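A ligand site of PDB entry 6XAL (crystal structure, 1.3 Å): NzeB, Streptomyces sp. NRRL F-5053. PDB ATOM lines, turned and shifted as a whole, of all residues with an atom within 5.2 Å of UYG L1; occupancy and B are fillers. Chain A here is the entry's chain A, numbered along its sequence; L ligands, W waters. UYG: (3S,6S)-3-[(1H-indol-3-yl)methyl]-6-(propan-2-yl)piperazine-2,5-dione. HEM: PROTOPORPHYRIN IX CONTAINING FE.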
ATOM      1  N   GLN A  75     -27.660  -4.649 -11.277  1.00  0.00           N
ATOM      2  CA  GLN A  75     -27.575  -5.340 -12.554  1.00  0.00           C
ATOM      3  C   GLN A  75     -26.134  -5.533 -13.008  1.00  0.00           C
ATOM      4  O   GLN A  75     -25.856  -6.494 -13.742  1.00  0.00           O
ATOM      5  CB  GLN A  75     -28.391  -4.599 -13.625  1.00  0.00           C
ATOM      6  CG  GLN A  75     -27.971  -3.163 -13.865  1.00  0.00           C
ATOM      7  CD  GLN A  75     -29.109  -2.261 -14.390  1.00  0.00           C
ATOM      8  OE1 GLN A  75     -29.593  -2.420 -15.521  1.00  0.00           O
ATOM      9  NE2 GLN A  75     -29.486  -1.264 -13.592  1.00  0.00           N
ATOM     10  N   GLU A  76     -25.203  -4.655 -12.598  1.00  0.00           N
ATOM     11  CA  GLU A  76     -23.842  -4.733 -13.104  1.00  0.00           C
ATOM     12  C   GLU A  76     -23.082  -5.892 -12.441  1.00  0.00           C
ATOM     13  O   GLU A  76     -23.282  -6.155 -11.253  1.00  0.00           O
ATOM     14  CB  GLU A  76     -23.089  -3.408 -12.874  1.00  0.00           C
ATOM     15  CG  GLU A  76     -22.902  -2.985 -11.415  1.00  0.00           C
ATOM     16  CD  GLU A  76     -24.019  -2.078 -10.906  1.00  0.00           C
ATOM     17  OE1 GLU A  76     -25.137  -2.109 -11.467  1.00  0.00           O
ATOM     18  OE2 GLU A  76     -23.768  -1.313  -9.942  1.00  0.00           O
ATOM     19  N   LEU A  80     -19.089  -0.603  -9.551  1.00  0.00           N
ATOM     20  CA  LEU A  80     -18.509   0.473 -10.347  1.00  0.00           C
ATOM     21  C   LEU A  80     -17.622   1.396  -9.510  1.00  0.00           C
ATOM     22  O   LEU A  80     -17.538   2.603  -9.782  1.00  0.00           O
ATOM     23  CB  LEU A  80     -19.599   1.263 -11.060  1.00  0.00           C
ATOM     24  CG  LEU A  80     -20.663   0.397 -11.736  1.00  0.00           C
ATOM     25  CD1 LEU A  80     -21.689   1.270 -12.449  1.00  0.00           C
ATOM     26  CD2 LEU A  80     -20.045  -0.616 -12.712  1.00  0.00           C
ATOM     27  N   PHE A 177     -21.401  -5.623 -19.286  1.00  0.00           N
ATOM     28  CA  PHE A 177     -22.110  -6.777 -18.707  1.00  0.00           C
ATOM     29  C   PHE A 177     -21.335  -8.079 -18.926  1.00  0.00           C
ATOM     30  O   PHE A 177     -21.475  -9.042 -18.171  1.00  0.00           O
ATOM     31  CB  PHE A 177     -23.519  -6.886 -19.312  1.00  0.00           C
ATOM     32  CG  PHE A 177     -24.499  -5.878 -18.771  1.00  0.00           C
ATOM     33  CD1 PHE A 177     -25.000  -5.994 -17.482  1.00  0.00           C
ATOM     34  CD2 PHE A 177     -24.929  -4.826 -19.566  1.00  0.00           C
ATOM     35  CE1 PHE A 177     -25.910  -5.078 -16.991  1.00  0.00           C
ATOM     36  CE2 PHE A 177     -25.841  -3.901 -19.079  1.00  0.00           C
ATOM     37  CZ  PHE A 177     -26.326  -4.023 -17.785  1.00  0.00           C
ATOM     38  N   THR A 244     -21.003   7.606 -22.883  1.00  0.00           N
ATOM     39  CA  THR A 244     -22.325   8.131 -23.245  1.00  0.00           C
ATOM     40  C   THR A 244     -22.218   8.988 -24.500  1.00  0.00           C
ATOM     41  O   THR A 244     -22.929   8.759 -25.480  1.00  0.00           O
ATOM     42  CB  THR A 244     -22.824   8.958 -22.066  1.00  0.00           C
ATOM     43  OG1 THR A 244     -21.772   9.858 -21.675  1.00  0.00           O
ATOM     44  CG2 THR A 244     -23.216   8.048 -20.903  1.00  0.00           C
ATOM     45  N   LEU A 286     -29.457   3.868 -26.201  1.00  0.00           N
ATOM     46  CA  LEU A 286     -28.121   4.069 -25.653  1.00  0.00           C
ATOM     47  C   LEU A 286     -27.745   2.973 -24.669  1.00  0.00           C
ATOM     48  O   LEU A 286     -27.036   2.030 -25.027  1.00  0.00           O
ATOM     49  CB  LEU A 286     -27.948   5.478 -25.070  1.00  0.00           C
ATOM     50  CG  LEU A 286     -26.519   5.796 -24.589  1.00  0.00           C
ATOM     51  CD1 LEU A 286     -25.441   5.584 -25.674  1.00  0.00           C
ATOM     52  CD2 LEU A 286     -26.444   7.199 -24.042  1.00  0.00           C
ATOM     53  N   SER A 287     -28.223   3.052 -23.430  1.00  0.00           N
ATOM     54  CA  SER A 287     -27.893   2.015 -22.463  1.00  0.00           C
ATOM     55  C   SER A 287     -28.558   0.694 -22.814  1.00  0.00           C
ATOM     56  O   SER A 287     -29.702   0.656 -23.270  1.00  0.00           O
ATOM     57  CB  SER A 287     -28.316   2.443 -21.061  1.00  0.00           C
ATOM     58  OG  SER A 287     -27.933   1.457 -20.108  1.00  0.00           O
ATOM     59  N   GLY A 289     -28.874  -1.436 -20.283  1.00  0.00           N
ATOM     60  CA  GLY A 289     -29.565  -1.725 -19.028  1.00  0.00           C
ATOM     61  C   GLY A 289     -30.570  -0.650 -18.686  1.00  0.00           C
ATOM     62  O   GLY A 289     -31.163  -0.055 -19.599  1.00  0.00           O
ATOM     63  N   SER A 290     -30.748  -0.353 -17.396  1.00  0.00           N
ATOM     64  CA  SER A 290     -31.814   0.523 -16.934  1.00  0.00           C
ATOM     65  C   SER A 290     -31.282   1.512 -15.894  1.00  0.00           C
ATOM     66  O   SER A 290     -30.326   1.223 -15.178  1.00  0.00           O
ATOM     67  CB  SER A 290     -32.926  -0.306 -16.273  1.00  0.00           C
ATOM     68  OG  SER A 290     -33.654  -1.058 -17.244  1.00  0.00           O
ATOM     69  N   VAL A 291     -31.930   2.682 -15.797  1.00  0.00           N
ATOM     70  CA  VAL A 291     -31.724   3.501 -14.601  1.00  0.00           C
ATOM     71  C   VAL A 291     -32.421   2.800 -13.452  1.00  0.00           C
ATOM     72  O   VAL A 291     -33.373   2.037 -13.655  1.00  0.00           O
ATOM     73  CB  VAL A 291     -32.187   4.967 -14.730  1.00  0.00           C
ATOM     74  CG1 VAL A 291     -31.661   5.638 -15.984  1.00  0.00           C
ATOM     75  CG2 VAL A 291     -33.620   5.070 -14.734  1.00  0.00           C
ATOM     76  N   LYS A 292     -31.927   3.017 -12.240  1.00  0.00           N
ATOM     77  CA  LYS A 292     -32.417   2.231 -11.121  1.00  0.00           C
ATOM     78  C   LYS A 292     -32.486   3.069  -9.849  1.00  0.00           C
ATOM     79  O   LYS A 292     -31.737   4.028  -9.671  1.00  0.00           O
ATOM     80  CB  LYS A 292     -31.605   0.940 -10.937  1.00  0.00           C
ATOM     81  CG  LYS A 292     -30.325   1.083 -10.149  1.00  0.00           C
ATOM     82  CD  LYS A 292     -29.278   1.905 -10.870  1.00  0.00           C
ATOM     83  CE  LYS A 292     -27.906   1.793 -10.215  1.00  0.00           C
ATOM     84  NZ  LYS A 292     -26.995   2.873 -10.690  1.00  0.00           N
ATOM     85  N   LEU A 316     -34.924   3.164 -20.250  1.00  0.00           N
ATOM     86  CA  LEU A 316     -35.260   4.405 -20.938  1.00  0.00           C
ATOM     87  C   LEU A 316     -35.657   4.106 -22.375  1.00  0.00           C
ATOM     88  O   LEU A 316     -36.549   4.765 -22.934  1.00  0.00           O
ATOM     89  CB  LEU A 316     -34.090   5.377 -20.893  1.00  0.00           C
ATOM     90  CG  LEU A 316     -33.552   5.670 -19.499  1.00  0.00           C
ATOM     91  CD1 LEU A 316     -32.426   6.666 -19.586  1.00  0.00           C
ATOM     92  CD2 LEU A 316     -34.659   6.231 -18.601  1.00  0.00           C
ATOM     93  N   GLY A 343     -34.565  10.287 -22.773  1.00  0.00           N
ATOM     94  CA  GLY A 343     -33.165  10.052 -23.091  1.00  0.00           C
ATOM     95  C   GLY A 343     -32.185  10.580 -22.058  1.00  0.00           C
ATOM     96  O   GLY A 343     -31.060  10.047 -21.946  1.00  0.00           O
ATOM     97  N   PHE A 390     -22.322  -1.376 -21.505  1.00  0.00           N
ATOM     98  CA  PHE A 390     -23.468  -0.661 -20.958  1.00  0.00           C
ATOM     99  C   PHE A 390     -24.016   0.326 -21.971  1.00  0.00           C
ATOM    100  O   PHE A 390     -25.236   0.487 -22.094  1.00  0.00           O
ATOM    101  CB  PHE A 390     -23.059   0.128 -19.711  1.00  0.00           C
ATOM    102  CG  PHE A 390     -22.723  -0.710 -18.484  1.00  0.00           C
ATOM    103  CD1 PHE A 390     -22.946  -2.075 -18.456  1.00  0.00           C
ATOM    104  CD2 PHE A 390     -22.219  -0.091 -17.355  1.00  0.00           C
ATOM    105  CE1 PHE A 390     -22.635  -2.819 -17.307  1.00  0.00           C
ATOM    106  CE2 PHE A 390     -21.905  -0.817 -16.219  1.00  0.00           C
ATOM    107  CZ  PHE A 390     -22.106  -2.179 -16.195  1.00  0.00           C
ATOM    108  N   PHE A 391     -23.129   1.029 -22.670  1.00  0.00           N
ATOM    109  CA  PHE A 391     -23.511   2.095 -23.590  1.00  0.00           C
ATOM    110  C   PHE A 391     -23.164   1.625 -24.994  1.00  0.00           C
ATOM    111  O   PHE A 391     -21.993   1.586 -25.374  1.00  0.00           O
ATOM    112  CB  PHE A 391     -22.822   3.388 -23.186  1.00  0.00           C
ATOM    113  CG  PHE A 391     -23.198   3.841 -21.805  1.00  0.00           C
ATOM    114  CD1 PHE A 391     -24.504   4.255 -21.538  1.00  0.00           C
ATOM    115  CD2 PHE A 391     -22.287   3.799 -20.766  1.00  0.00           C
ATOM    116  CE1 PHE A 391     -24.873   4.648 -20.250  1.00  0.00           C
ATOM    117  CE2 PHE A 391     -22.662   4.188 -19.484  1.00  0.00           C
ATOM    118  CZ  PHE A 391     -23.938   4.605 -19.228  1.00  0.00           C
HETATM  119  C10 UYG L   1     -27.903   6.793 -20.336  1.00  0.00           C
HETATM  120  C11 UYG L   1     -25.409   1.260 -15.897  1.00  0.00           C
HETATM  121  C12 UYG L   1     -25.764  -0.215 -16.106  1.00  0.00           C
HETATM  122  C13 UYG L   1     -25.391  -1.054 -14.877  1.00  0.00           C
HETATM  123  N   UYG L   1     -29.412   4.926 -19.373  1.00  0.00           N
HETATM  124  C   UYG L   1     -26.794   3.038 -14.635  1.00  0.00           C
HETATM  125  O   UYG L   1     -27.253   3.383 -13.596  1.00  0.00           O
HETATM  126  C1  UYG L   1     -26.979   3.901 -15.891  1.00  0.00           C
HETATM  127  C14 UYG L   1     -27.254  -0.350 -16.405  1.00  0.00           C
HETATM  128  C15 UYG L   1     -25.858   1.972 -17.174  1.00  0.00           C
HETATM  129  C2  UYG L   1     -28.426   4.415 -16.047  1.00  0.00           C
HETATM  130  C3  UYG L   1     -28.669   4.862 -17.518  1.00  0.00           C
HETATM  131  C4  UYG L   1     -29.575   4.293 -18.266  1.00  0.00           C
HETATM  132  C5  UYG L   1     -28.437   5.895 -19.433  1.00  0.00           C
HETATM  133  C6  UYG L   1     -27.900   5.853 -18.071  1.00  0.00           C
HETATM  134  C7  UYG L   1     -26.864   6.699 -17.717  1.00  0.00           C
HETATM  135  C8  UYG L   1     -26.331   7.610 -18.641  1.00  0.00           C
HETATM  136  C9  UYG L   1     -26.852   7.630 -19.960  1.00  0.00           C
HETATM  137  N1  UYG L   1     -26.590   3.217 -17.115  1.00  0.00           N
HETATM  138  N2  UYG L   1     -26.047   1.788 -14.688  1.00  0.00           N
HETATM  139  O1  UYG L   1     -25.598   1.508 -18.246  1.00  0.00           O
HETATM  140  CHA HEM L   2     -27.003  11.316 -15.607  1.00  0.00           C
HETATM  141  CHB HEM L   2     -27.931  10.518 -20.316  1.00  0.00           C
HETATM  142  CHC HEM L   2     -23.889  12.920 -21.484  1.00  0.00           C
HETATM  143  CHD HEM L   2     -22.976  13.727 -16.798  1.00  0.00           C
HETATM  144  C1A HEM L   2     -27.642  10.913 -16.754  1.00  0.00           C
HETATM  145  C2A HEM L   2     -28.876  10.175 -16.838  1.00  0.00           C
HETATM  146  C3A HEM L   2     -29.105   9.952 -18.140  1.00  0.00           C
HETATM  147  C4A HEM L   2     -28.045  10.536 -18.932  1.00  0.00           C
HETATM  148  CMA HEM L   2     -30.296   9.208 -18.743  1.00  0.00           C
HETATM  149  CAA HEM L   2     -29.794   9.756 -15.657  1.00  0.00           C
HETATM  150  CBA HEM L   2     -29.360   8.502 -14.949  1.00  0.00           C
HETATM  151  CGA HEM L   2     -30.299   8.195 -13.807  1.00  0.00           C
HETATM  152  O1A HEM L   2     -31.445   8.717 -13.773  1.00  0.00           O
HETATM  153  O2A HEM L   2     -29.879   7.413 -12.919  1.00  0.00           O
HETATM  154  C1B HEM L   2     -26.922  11.077 -21.057  1.00  0.00           C
HETATM  155  C2B HEM L   2     -26.813  11.099 -22.502  1.00  0.00           C
HETATM  156  C3B HEM L   2     -25.675  11.747 -22.815  1.00  0.00           C
HETATM  157  C4B HEM L   2     -25.056  12.184 -21.577  1.00  0.00           C
HETATM  158  CMB HEM L   2     -27.847  10.440 -23.445  1.00  0.00           C
HETATM  159  CAB HEM L   2     -25.079  12.065 -24.209  1.00  0.00           C
HETATM  160  CBB HEM L   2     -25.766  11.995 -25.356  1.00  0.00           C
HETATM  161  C1C HEM L   2     -23.297  13.374 -20.321  1.00  0.00           C
HETATM  162  C2C HEM L   2     -22.054  14.116 -20.259  1.00  0.00           C
HETATM  163  C3C HEM L   2     -21.799  14.325 -18.953  1.00  0.00           C
HETATM  164  C4C HEM L   2     -22.856  13.736 -18.174  1.00  0.00           C
HETATM  165  CMC HEM L   2     -21.208  14.569 -21.477  1.00  0.00           C
HETATM  166  CAC HEM L   2     -20.578  15.094 -18.414  1.00  0.00           C
HETATM  167  CBC HEM L   2     -19.946  14.665 -17.314  1.00  0.00           C
HETATM  168  C1D HEM L   2     -23.936  13.085 -16.070  1.00  0.00           C
HETATM  169  C2D HEM L   2     -23.939  12.884 -14.636  1.00  0.00           C
HETATM  170  C3D HEM L   2     -25.039  12.222 -14.301  1.00  0.00           C
HETATM  171  C4D HEM L   2     -25.785  11.961 -15.524  1.00  0.00           C
HETATM  172  CMD HEM L   2     -22.820  13.384 -13.699  1.00  0.00           C
HETATM  173  CAD HEM L   2     -25.442  11.767 -12.867  1.00  0.00           C
HETATM  174  CBD HEM L   2     -26.558  12.620 -12.301  1.00  0.00           C
HETATM  175  CGD HEM L   2     -27.157  11.979 -11.066  1.00  0.00           C
HETATM  176  O1D HEM L   2     -27.042  10.732 -10.873  1.00  0.00           O
HETATM  177  O2D HEM L   2     -27.742  12.760 -10.291  1.00  0.00           O
HETATM  178  NA  HEM L   2     -27.159  11.115 -18.040  1.00  0.00           N
HETATM  179  NB  HEM L   2     -25.850  11.763 -20.498  1.00  0.00           N
HETATM  180  NC  HEM L   2     -23.769  13.162 -19.037  1.00  0.00           N
HETATM  181  ND  HEM L   2     -25.092  12.493 -16.596  1.00  0.00           N
HETATM  182 FE   HEM L   2     -25.603  12.372 -18.578  1.00  0.00          FE
HETATM  183  C10 UYG L   3     -22.766   6.014 -16.177  1.00  0.00           C
HETATM  184  C11 UYG L   3     -22.753   7.707 -10.387  1.00  0.00           C
HETATM  185  C12 UYG L   3     -21.540   7.827 -11.315  1.00  0.00           C
HETATM  186  C13 UYG L   3     -21.953   7.945 -12.783  1.00  0.00           C
HETATM  187  N   UYG L   3     -24.332   7.924 -15.451  1.00  0.00           N
HETATM  188  C   UYG L   3     -24.635   6.006 -10.855  1.00  0.00           C
HETATM  189  O   UYG L   3     -24.993   4.864 -10.877  1.00  0.00           O
HETATM  190  C1  UYG L   3     -25.629   7.095 -11.254  1.00  0.00           C
HETATM  191  C14 UYG L   3     -20.647   6.596 -11.141  1.00  0.00           C
HETATM  192  C15 UYG L   3     -23.806   8.787 -10.643  1.00  0.00           C
HETATM  193  C2  UYG L   3     -26.164   6.855 -12.682  1.00  0.00           C
HETATM  194  C3  UYG L   3     -25.196   7.036 -13.880  1.00  0.00           C
HETATM  195  C4  UYG L   3     -25.211   8.140 -14.553  1.00  0.00           C
HETATM  196  C5  UYG L   3     -23.723   6.688 -15.440  1.00  0.00           C
HETATM  197  C6  UYG L   3     -24.366   6.038 -14.306  1.00  0.00           C
HETATM  198  C7  UYG L   3     -24.012   4.753 -13.974  1.00  0.00           C
HETATM  199  C8  UYG L   3     -23.038   4.078 -14.722  1.00  0.00           C
HETATM  200  C9  UYG L   3     -22.423   4.711 -15.826  1.00  0.00           C
HETATM  201  N1  UYG L   3     -25.154   8.453 -11.076  1.00  0.00           N
HETATM  202  N2  UYG L   3     -23.285   6.352 -10.472  1.00  0.00           N
HETATM  203  O1  UYG L   3     -23.514   9.932 -10.522  1.00  0.00           O
HETATM  204  O   HOH W   1     -29.436   4.786 -12.550  1.00  0.00           O
HETATM  205  O   HOH W   2     -32.016   2.595 -20.071  1.00  0.00           O
HETATM  206  O   HOH W   3     -25.188   0.895 -12.067  1.00  0.00           O
HETATM  207  O   HOH W   4     -23.958   9.928 -17.731  1.00  0.00           O
HETATM  208  O   HOH W   5     -30.190   5.061 -22.285  1.00  0.00           O
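An oxygen (O) of UYG L1 is in hydrogen-bond range of the side-chain amino group (NZ) of Lys 292, at 3.0 Å.
The side-chain hydroxyl of Ser 287 lies within hydrogen-bond range of an oxygen (O1) of UYG L1, 3.0 Å away.
NZ of Lys 292 lies within hydrogen-bond range of O of UYG L3.
An oxygen (O1D) of HEM L2 lies within hydrogen-bond range of a nitrogen (N1) of UYG L3 (3.0 Å).
OG of Ser 287 sits close to O of Phe 390 (3.5 Å).
The side-chain hydroxyl (OG) of Ser 287 sits at hydrogen-bond distance from the backbone NH (N) of Gly 289 (3.0 Å).
OE1 of Gln 75 sits at hydrogen-bond distance from N of Ser 290, at 3.0 Å.
Merely in contact with UYG L1: Phe 390 (3.2 Å), Gln 75 (3.2 Å), Val 291 (3.4 Å), Leu 316 (3.5 Å), Glu 76 (3.6 Å), Phe 391 (3.6 Å), Ser 290 (3.6 Å), Gly 289 (3.8 Å) and Thr 244 (3.8 Å).
Within 4 Å of UYG L1: Gln 75, Glu 76, Thr 244, Ser 287, Gly 289, Ser 290, Val 291, Lys 292, Leu 316, Phe 390 and Phe 391.
The nearest printed residue that does not touch UYG L1 is Leu 286 (4.003 Å).
Water W1 lies within hydrogen-bond range of an oxygen (O2A) of HEM L2 (2.7 Å), an oxygen (O) of UYG L1 (2.8 Å) and the backbone NH (N) of Lys 292 (3.1 Å).
Water W3 lies within hydrogen-bond range of a nitrogen (N2) of UYG L1 (2.9 Å), the side-chain amino group (NZ) of Lys 292 (3.0 Å) and the side-chain carboxylate (OE1) of Glu 76 (3.1 Å).
Water W5 lies within hydrogen-bond range of a nitrogen (N) of UYG L1 and the backbone NH (N) of Ser 287.
Water W2 lies within hydrogen-bond range of O of Gly 289 (2.8 Å) and N of Leu 316 (3.0 Å).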
